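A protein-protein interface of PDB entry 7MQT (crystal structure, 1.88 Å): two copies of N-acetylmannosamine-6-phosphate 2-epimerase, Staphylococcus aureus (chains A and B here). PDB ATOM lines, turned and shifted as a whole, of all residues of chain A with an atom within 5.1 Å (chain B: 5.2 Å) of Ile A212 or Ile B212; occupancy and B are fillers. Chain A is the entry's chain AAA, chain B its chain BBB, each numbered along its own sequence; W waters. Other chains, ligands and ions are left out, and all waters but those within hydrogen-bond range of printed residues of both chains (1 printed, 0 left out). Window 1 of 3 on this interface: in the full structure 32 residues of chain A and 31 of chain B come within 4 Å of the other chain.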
ATOM      1  N   GLY A 204      28.050  26.424  -8.055  1.00  0.00           N
ATOM      2  CA  GLY A 204      28.126  25.351  -9.068  1.00  0.00           C
ATOM      3  C   GLY A 204      26.966  24.362  -9.022  1.00  0.00           C
ATOM      4  O   GLY A 204      26.521  23.949 -10.108  1.00  0.00           O
ATOM      5  N   ALA A 205      26.465  24.016  -7.830  1.00  0.00           N
ATOM      6  CA  ALA A 205      25.370  23.037  -7.644  1.00  0.00           C
ATOM      7  C   ALA A 205      24.043  23.581  -8.209  1.00  0.00           C
ATOM      8  O   ALA A 205      23.149  22.743  -8.470  1.00  0.00           O
ATOM      9  CB  ALA A 205      25.241  22.656  -6.198  1.00  0.00           C
ATOM     10  N   ILE A 206      23.945  24.883  -8.456  1.00  0.00           N
ATOM     11  CA  ILE A 206      22.702  25.541  -8.996  1.00  0.00           C
ATOM     12  C   ILE A 206      22.927  26.177 -10.369  1.00  0.00           C
ATOM     13  O   ILE A 206      22.038  26.004 -11.254  1.00  0.00           O
ATOM     14  CB  ILE A 206      22.124  26.546  -8.001  1.00  0.00           C
ATOM     15  CG1 ILE A 206      21.838  25.849  -6.674  1.00  0.00           C
ATOM     16  CG2 ILE A 206      20.881  27.260  -8.572  1.00  0.00           C
ATOM     17  CD1 ILE A 206      21.374  26.768  -5.594  1.00  0.00           C
ATOM     18  N   THR A 207      24.048  26.869 -10.565  1.00  0.00           N
ATOM     19  CA  THR A 207      24.253  27.736 -11.733  1.00  0.00           C
ATOM     20  C   THR A 207      25.386  27.268 -12.641  1.00  0.00           C
ATOM     21  O   THR A 207      25.694  28.044 -13.594  1.00  0.00           O
ATOM     22  CB  THR A 207      24.463  29.185 -11.289  1.00  0.00           C
ATOM     23  OG1 THR A 207      25.651  29.192 -10.520  1.00  0.00           O
ATOM     24  CG2 THR A 207      23.288  29.702 -10.494  1.00  0.00           C
ATOM     25  N   ARG A 208      25.923  26.056 -12.463  1.00  0.00           N
ATOM     26  CA  ARG A 208      26.952  25.546 -13.391  1.00  0.00           C
ATOM     27  C   ARG A 208      26.523  24.175 -13.904  1.00  0.00           C
ATOM     28  O   ARG A 208      26.962  23.141 -13.422  1.00  0.00           O
ATOM     29  CB  ARG A 208      28.306  25.512 -12.697  1.00  0.00           C
ATOM     30  CG  ARG A 208      28.912  26.889 -12.482  1.00  0.00           C
ATOM     31  CD  ARG A 208      30.385  26.751 -12.121  1.00  0.00           C
ATOM     32  NE  ARG A 208      31.040  27.994 -12.433  1.00  0.00           N
ATOM     33  CZ  ARG A 208      31.535  28.853 -11.533  1.00  0.00           C
ATOM     34  NH1 ARG A 208      31.487  28.577 -10.231  1.00  0.00           N
ATOM     35  NH2 ARG A 208      32.099  29.983 -11.948  1.00  0.00           N
ATOM     36  N   PRO A 209      25.626  24.143 -14.893  1.00  0.00           N
ATOM     37  CA  PRO A 209      25.116  22.896 -15.427  1.00  0.00           C
ATOM     38  C   PRO A 209      26.254  21.955 -15.837  1.00  0.00           C
ATOM     39  O   PRO A 209      26.052  20.728 -15.754  1.00  0.00           O
ATOM     40  CB  PRO A 209      24.225  23.337 -16.584  1.00  0.00           C
ATOM     41  CG  PRO A 209      24.615  24.758 -16.873  1.00  0.00           C
ATOM     42  CD  PRO A 209      25.070  25.320 -15.553  1.00  0.00           C
ATOM     43  N   LYS A 210      27.407  22.468 -16.286  1.00  0.00           N
ATOM     44  CA  LYS A 210      28.525  21.555 -16.673  1.00  0.00           C
ATOM     45  C   LYS A 210      28.974  20.793 -15.427  1.00  0.00           C
ATOM     46  O   LYS A 210      29.200  19.574 -15.518  1.00  0.00           O
ATOM     47  CB  LYS A 210      29.680  22.330 -17.311  1.00  0.00           C
ATOM     48  CG  LYS A 210      30.997  21.576 -17.432  1.00  0.00           C
ATOM     49  CD  LYS A 210      32.117  22.454 -17.957  1.00  0.00           C
ATOM     50  CE  LYS A 210      33.446  21.736 -18.087  1.00  0.00           C
ATOM     51  NZ  LYS A 210      34.292  22.414 -19.102  1.00  0.00           N
ATOM     52  N   GLU A 211      29.085  21.465 -14.295  1.00  0.00           N
ATOM     53  CA  GLU A 211      29.586  20.833 -13.050  1.00  0.00           C
ATOM     54  C   GLU A 211      28.542  19.850 -12.524  1.00  0.00           C
ATOM     55  O   GLU A 211      28.920  18.763 -12.045  1.00  0.00           O
ATOM     56  CB  GLU A 211      29.907  21.897 -12.010  1.00  0.00           C
ATOM     57  CG  GLU A 211      31.012  22.833 -12.459  1.00  0.00           C
ATOM     58  CD  GLU A 211      31.655  23.614 -11.329  1.00  0.00           C
ATOM     59  OE1 GLU A 211      31.121  23.542 -10.165  1.00  0.00           O
ATOM     60  OE2 GLU A 211      32.673  24.279 -11.604  1.00  0.00           O
ATOM     61  N   ILE A 212      27.262  20.198 -12.643  1.00  0.00           N
ATOM     62  CA  ILE A 212      26.179  19.298 -12.161  1.00  0.00           C
ATOM     63  C   ILE A 212      26.183  18.082 -13.068  1.00  0.00           C
ATOM     64  O   ILE A 212      26.144  16.967 -12.562  1.00  0.00           O
ATOM     65  CB  ILE A 212      24.793  19.968 -12.171  1.00  0.00           C
ATOM     66  CG1 ILE A 212      24.835  21.321 -11.457  1.00  0.00           C
ATOM     67  CG2 ILE A 212      23.766  19.029 -11.568  1.00  0.00           C
ATOM     68  CD1 ILE A 212      23.587  22.135 -11.652  1.00  0.00           C
ATOM     69  N   THR A 213      26.273  18.303 -14.383  1.00  0.00           N
ATOM     70  CA  THR A 213      26.315  17.186 -15.354  1.00  0.00           C
ATOM     71  C   THR A 213      27.456  16.242 -14.963  1.00  0.00           C
ATOM     72  O   THR A 213      27.257  15.006 -14.946  1.00  0.00           O
ATOM     73  CB  THR A 213      26.499  17.701 -16.780  1.00  0.00           C
ATOM     74  OG1 THR A 213      25.398  18.555 -17.111  1.00  0.00           O
ATOM     75  CG2 THR A 213      26.619  16.558 -17.758  1.00  0.00           C
ATOM     76  N   LYS A 214      28.631  16.788 -14.687  1.00  0.00           N
ATOM     77  CA  LYS A 214      29.823  15.963 -14.327  1.00  0.00           C
ATOM     78  C   LYS A 214      29.533  15.097 -13.113  1.00  0.00           C
ATOM     79  O   LYS A 214      30.022  13.960 -13.103  1.00  0.00           O
ATOM     80  CB  LYS A 214      31.061  16.818 -14.066  1.00  0.00           C
ATOM     81  CG  LYS A 214      31.714  17.322 -15.339  1.00  0.00           C
ATOM     82  CD  LYS A 214      32.688  18.465 -15.120  1.00  0.00           C
ATOM     83  CE  LYS A 214      33.963  18.058 -14.414  1.00  0.00           C
ATOM     84  NZ  LYS A 214      34.658  19.248 -13.853  1.00  0.00           N
ATOM     85  N   ARG A 215      28.774  15.588 -12.123  1.00  0.00           N
ATOM     86  CA  ARG A 215      28.458  14.780 -10.919  1.00  0.00           C
ATOM     87  C   ARG A 215      27.538  13.618 -11.277  1.00  0.00           C
ATOM     88  O   ARG A 215      27.728  12.524 -10.723  1.00  0.00           O
ATOM     89  CB  ARG A 215      27.799  15.625  -9.837  1.00  0.00           C
ATOM     90  CG  ARG A 215      28.763  16.557  -9.125  1.00  0.00           C
ATOM     91  CD  ARG A 215      28.199  16.972  -7.777  1.00  0.00           C
ATOM     92  NE  ARG A 215      27.344  18.151  -7.829  1.00  0.00           N
ATOM     93  CZ  ARG A 215      26.053  18.226  -7.455  1.00  0.00           C
ATOM     94  NH1 ARG A 215      25.375  17.177  -7.013  1.00  0.00           N
ATOM     95  NH2 ARG A 215      25.445  19.397  -7.519  1.00  0.00           N
ATOM     96  N   PHE A 216      26.557  13.853 -12.152  1.00  0.00           N
ATOM     97  CA  PHE A 216      25.712  12.762 -12.673  1.00  0.00           C
ATOM     98  C   PHE A 216      26.615  11.769 -13.393  1.00  0.00           C
ATOM     99  O   PHE A 216      26.531  10.570 -13.147  1.00  0.00           O
ATOM    100  CB  PHE A 216      24.593  13.304 -13.569  1.00  0.00           C
ATOM    101  CG  PHE A 216      23.405  13.782 -12.780  1.00  0.00           C
ATOM    102  CD1 PHE A 216      23.390  15.051 -12.252  1.00  0.00           C
ATOM    103  CD2 PHE A 216      22.313  12.969 -12.556  1.00  0.00           C
ATOM    104  CE1 PHE A 216      22.317  15.496 -11.497  1.00  0.00           C
ATOM    105  CE2 PHE A 216      21.235  13.407 -11.802  1.00  0.00           C
ATOM    106  CZ  PHE A 216      21.247  14.673 -11.267  1.00  0.00           C
ATOM    107  N   GLY B 204      15.541  19.136 -14.967  1.00  0.00           N
ATOM    108  CA  GLY B 204      15.544  20.227 -13.968  1.00  0.00           C
ATOM    109  C   GLY B 204      16.706  20.178 -13.005  1.00  0.00           C
ATOM    110  O   GLY B 204      17.175  21.268 -12.587  1.00  0.00           O
ATOM    111  N   ALA B 205      17.177  18.989 -12.662  1.00  0.00           N
ATOM    112  CA  ALA B 205      18.312  18.827 -11.735  1.00  0.00           C
ATOM    113  C   ALA B 205      19.582  19.476 -12.305  1.00  0.00           C
ATOM    114  O   ALA B 205      20.541  19.718 -11.531  1.00  0.00           O
ATOM    115  CB  ALA B 205      18.537  17.363 -11.456  1.00  0.00           C
ATOM    116  N   ILE B 206      19.653  19.649 -13.613  1.00  0.00           N
ATOM    117  CA  ILE B 206      20.829  20.261 -14.276  1.00  0.00           C
ATOM    118  C   ILE B 206      20.512  21.656 -14.825  1.00  0.00           C
ATOM    119  O   ILE B 206      21.333  22.579 -14.615  1.00  0.00           O
ATOM    120  CB  ILE B 206      21.391  19.311 -15.339  1.00  0.00           C
ATOM    121  CG1 ILE B 206      21.891  18.016 -14.680  1.00  0.00           C
ATOM    122  CG2 ILE B 206      22.492  20.036 -16.116  1.00  0.00           C
ATOM    123  CD1 ILE B 206      22.249  16.905 -15.666  1.00  0.00           C
ATOM    124  N   THR B 207      19.354  21.843 -15.463  1.00  0.00           N
ATOM    125  CA  THR B 207      19.109  23.010 -16.313  1.00  0.00           C
ATOM    126  C   THR B 207      18.004  23.928 -15.776  1.00  0.00           C
ATOM    127  O   THR B 207      17.738  24.930 -16.446  1.00  0.00           O
ATOM    128  CB  THR B 207      18.795  22.551 -17.730  1.00  0.00           C
ATOM    129  OG1 THR B 207      17.587  21.804 -17.678  1.00  0.00           O
ATOM    130  CG2 THR B 207      19.952  21.774 -18.318  1.00  0.00           C
ATOM    131  N   ARG B 208      17.432  23.633 -14.616  1.00  0.00           N
ATOM    132  CA  ARG B 208      16.419  24.522 -13.988  1.00  0.00           C
ATOM    133  C   ARG B 208      16.915  25.008 -12.634  1.00  0.00           C
ATOM    134  O   ARG B 208      16.563  24.455 -11.592  1.00  0.00           O
ATOM    135  CB  ARG B 208      15.069  23.841 -13.850  1.00  0.00           C
ATOM    136  CG  ARG B 208      14.366  23.587 -15.171  1.00  0.00           C
ATOM    137  CD  ARG B 208      12.913  23.132 -15.006  1.00  0.00           C
ATOM    138  NE  ARG B 208      12.211  23.286 -16.269  1.00  0.00           N
ATOM    139  CZ  ARG B 208      11.733  22.310 -17.056  1.00  0.00           C
ATOM    140  NH1 ARG B 208      11.831  21.024 -16.736  1.00  0.00           N
ATOM    141  NH2 ARG B 208      11.113  22.654 -18.174  1.00  0.00           N
ATOM    142  N   PRO B 209      17.742  26.082 -12.610  1.00  0.00           N
ATOM    143  CA  PRO B 209      18.272  26.598 -11.351  1.00  0.00           C
ATOM    144  C   PRO B 209      17.143  26.916 -10.355  1.00  0.00           C
ATOM    145  O   PRO B 209      17.354  26.807  -9.175  1.00  0.00           O
ATOM    146  CB  PRO B 209      19.057  27.851 -11.778  1.00  0.00           C
ATOM    147  CG  PRO B 209      18.541  28.182 -13.162  1.00  0.00           C
ATOM    148  CD  PRO B 209      18.255  26.818 -13.766  1.00  0.00           C
ATOM    149  N   LYS B 210      15.966  27.329 -10.833  1.00  0.00           N
ATOM    150  CA  LYS B 210      14.828  27.586  -9.921  1.00  0.00           C
ATOM    151  C   LYS B 210      14.505  26.305  -9.162  1.00  0.00           C
ATOM    152  O   LYS B 210      14.282  26.365  -7.926  1.00  0.00           O
ATOM    153  CB  LYS B 210      13.603  28.051 -10.693  1.00  0.00           C
ATOM    154  CG  LYS B 210      12.365  28.278  -9.856  1.00  0.00           C
ATOM    155  CD  LYS B 210      11.261  28.770 -10.745  1.00  0.00           C
ATOM    156  CE  LYS B 210       9.931  28.876 -10.032  1.00  0.00           C
ATOM    157  NZ  LYS B 210       8.987  29.725 -10.810  1.00  0.00           N
ATOM    158  N   GLU B 211      14.407  25.186  -9.880  1.00  0.00           N
ATOM    159  CA  GLU B 211      14.021  23.886  -9.276  1.00  0.00           C
ATOM    160  C   GLU B 211      15.128  23.440  -8.328  1.00  0.00           C
ATOM    161  O   GLU B 211      14.819  22.929  -7.228  1.00  0.00           O
ATOM    162  CB  GLU B 211      13.729  22.848 -10.358  1.00  0.00           C
ATOM    163  CG  GLU B 211      12.539  23.249 -11.211  1.00  0.00           C
ATOM    164  CD  GLU B 211      11.885  22.133 -12.011  1.00  0.00           C
ATOM    165  OE1 GLU B 211      12.483  21.025 -12.105  1.00  0.00           O
ATOM    166  OE2 GLU B 211      10.787  22.386 -12.543  1.00  0.00           O
ATOM    167  N   ILE B 212      16.370  23.621  -8.739  1.00  0.00           N
ATOM    168  CA  ILE B 212      17.485  23.177  -7.855  1.00  0.00           C
ATOM    169  C   ILE B 212      17.466  24.065  -6.607  1.00  0.00           C
ATOM    170  O   ILE B 212      17.621  23.535  -5.493  1.00  0.00           O
ATOM    171  CB  ILE B 212      18.847  23.221  -8.540  1.00  0.00           C
ATOM    172  CG1 ILE B 212      18.871  22.468  -9.861  1.00  0.00           C
ATOM    173  CG2 ILE B 212      19.911  22.691  -7.578  1.00  0.00           C
ATOM    174  CD1 ILE B 212      20.005  22.873 -10.743  1.00  0.00           C
ATOM    175  N   THR B 213      17.299  25.381  -6.781  1.00  0.00           N
ATOM    176  CA  THR B 213      17.242  26.311  -5.635  1.00  0.00           C
ATOM    177  C   THR B 213      16.147  25.844  -4.657  1.00  0.00           C
ATOM    178  O   THR B 213      16.419  25.766  -3.464  1.00  0.00           O
ATOM    179  CB  THR B 213      17.012  27.751  -6.094  1.00  0.00           C
ATOM    180  OG1 THR B 213      18.137  28.113  -6.886  1.00  0.00           O
ATOM    181  CG2 THR B 213      16.809  28.671  -4.914  1.00  0.00           C
ATOM    182  N   LYS B 214      14.955  25.518  -5.158  1.00  0.00           N
ATOM    183  CA  LYS B 214      13.816  25.079  -4.319  1.00  0.00           C
ATOM    184  C   LYS B 214      14.220  23.871  -3.462  1.00  0.00           C
ATOM    185  O   LYS B 214      13.819  23.829  -2.289  1.00  0.00           O
ATOM    186  CB  LYS B 214      12.592  24.756  -5.174  1.00  0.00           C
ATOM    187  CG  LYS B 214      11.795  25.952  -5.665  1.00  0.00           C
ATOM    188  CD  LYS B 214      10.523  25.545  -6.380  1.00  0.00           C
ATOM    189  CE  LYS B 214       9.649  26.729  -6.764  1.00  0.00           C
ATOM    190  NZ  LYS B 214       8.814  26.429  -7.961  1.00  0.00           N
ATOM    191  N   ARG B 215      14.946  22.897  -4.001  1.00  0.00           N
ATOM    192  CA  ARG B 215      15.341  21.694  -3.230  1.00  0.00           C
ATOM    193  C   ARG B 215      16.336  22.093  -2.121  1.00  0.00           C
ATOM    194  O   ARG B 215      16.254  21.530  -1.024  1.00  0.00           O
ATOM    195  CB  ARG B 215      15.917  20.640  -4.176  1.00  0.00           C
ATOM    196  CG  ARG B 215      14.907  20.124  -5.186  1.00  0.00           C
ATOM    197  CD  ARG B 215      15.348  18.821  -5.839  1.00  0.00           C
ATOM    198  NE  ARG B 215      16.274  19.036  -6.935  1.00  0.00           N
ATOM    199  CZ  ARG B 215      17.556  18.635  -6.970  1.00  0.00           C
ATOM    200  NH1 ARG B 215      18.114  17.984  -5.962  1.00  0.00           N
ATOM    201  NH2 ARG B 215      18.278  18.861  -8.051  1.00  0.00           N
ATOM    202  N   PHE B 216      17.229  23.034  -2.389  1.00  0.00           N
ATOM    203  CA  PHE B 216      18.142  23.539  -1.331  1.00  0.00           C
ATOM    204  C   PHE B 216      17.297  24.211  -0.254  1.00  0.00           C
ATOM    205  O   PHE B 216      17.504  23.911   0.900  1.00  0.00           O
ATOM    206  CB  PHE B 216      19.199  24.506  -1.858  1.00  0.00           C
ATOM    207  CG  PHE B 216      20.427  23.814  -2.388  1.00  0.00           C
ATOM    208  CD1 PHE B 216      20.424  23.241  -3.641  1.00  0.00           C
ATOM    209  CD2 PHE B 216      21.576  23.710  -1.623  1.00  0.00           C
ATOM    210  CE1 PHE B 216      21.547  22.584  -4.130  1.00  0.00           C
ATOM    211  CE2 PHE B 216      22.706  23.089  -2.125  1.00  0.00           C
ATOM    212  CZ  PHE B 216      22.677  22.496  -3.355  1.00  0.00           C
HETATM  213  O   HOH W   1      21.685  25.316 -13.990  1.00  0.00           O
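Water W1 lies within hydrogen-bond range of O of Ile B206 (2.8 Å) and O of Ile A206 (2.8 Å).
Ala A205 touches Ile B212, and with the chains exchanged Ile A212 touches Ala B205. Ala A205 touches Phe B216, and with the chains exchanged Phe A216 touches Ala B205. Ile A206 touches Ile B212, and with the chains exchanged Ile A212 touches Ile B206. Ile A212 touches its own counterpart, Ile B212. 13 positions are printed for both chains. Of the 11 pairs that touch across the chains among the printed residues, 11 have their exchanged pair printed and touching as well.
O of Ala A205 touches CG2 of Ile B212 (3.4 Å). Phe B216 touches Ala A205 (CZ to CB, 3.8 Å). Pro B209 touches Ile A206. O of Ile A206 touches CD1 of Ile B212, at 3.8 Å. OG1 of Thr B213 touches CG2 of Ile A206 (3.3 Å). Ile B206 touches Pro A209. Ile A212 touches Ile B206 (CD1 to O, 3.7 Å). Ile A212 touches Ile B212 (CD1 to CD1, 3.8 Å). Thr A213 touches Ile B206 (OG1 to CG2, 3.4 Å). CB of Ala B205 touches CZ of Phe A216, at 3.8 Å.
Of the 13 printed residues of chain B, 6 touch a printed residue of chain A. Printed residues of chain B that touch a printed residue of chain A: Ala B205, Ile B206, Pro B209, Ile B212, Thr B213 and Phe B216. Hydrophobic or aromatic side chains of chain B that line the printed part of chain A: Ala B205, Ile B206, Pro B209, Ile B212 and Phe B216.
O of Pro A209 is in hydrogen-bond range of OG1 of Thr A213 (2.6 Å). O of Pro B209 lies within hydrogen-bond range of OG1 of Thr B213 (2.7 Å).
Ile A212 touches just these residues of chain B: Ala B205, Ile B206 and Ile B212. Of chain A, only Ala A205, Ile A206 and Ile A212 come within 4 Å of Ile B212. Of the printed residues of chain A, Ala B205 touches Ile A212 (3.3 Å) and Phe A216 (3.8 Å). Printed residues of chain B within 4 Å of Pro A209: Ile B206 (3.6 Å). Of the printed residues of chain A, Pro B209 touches Ile A206 (3.5 Å). Lys A214 touches none of the printed residues of chain B. The nearest printed residue of chain A that does not touch Ala B205 is Ala A205 (5.0 Å).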
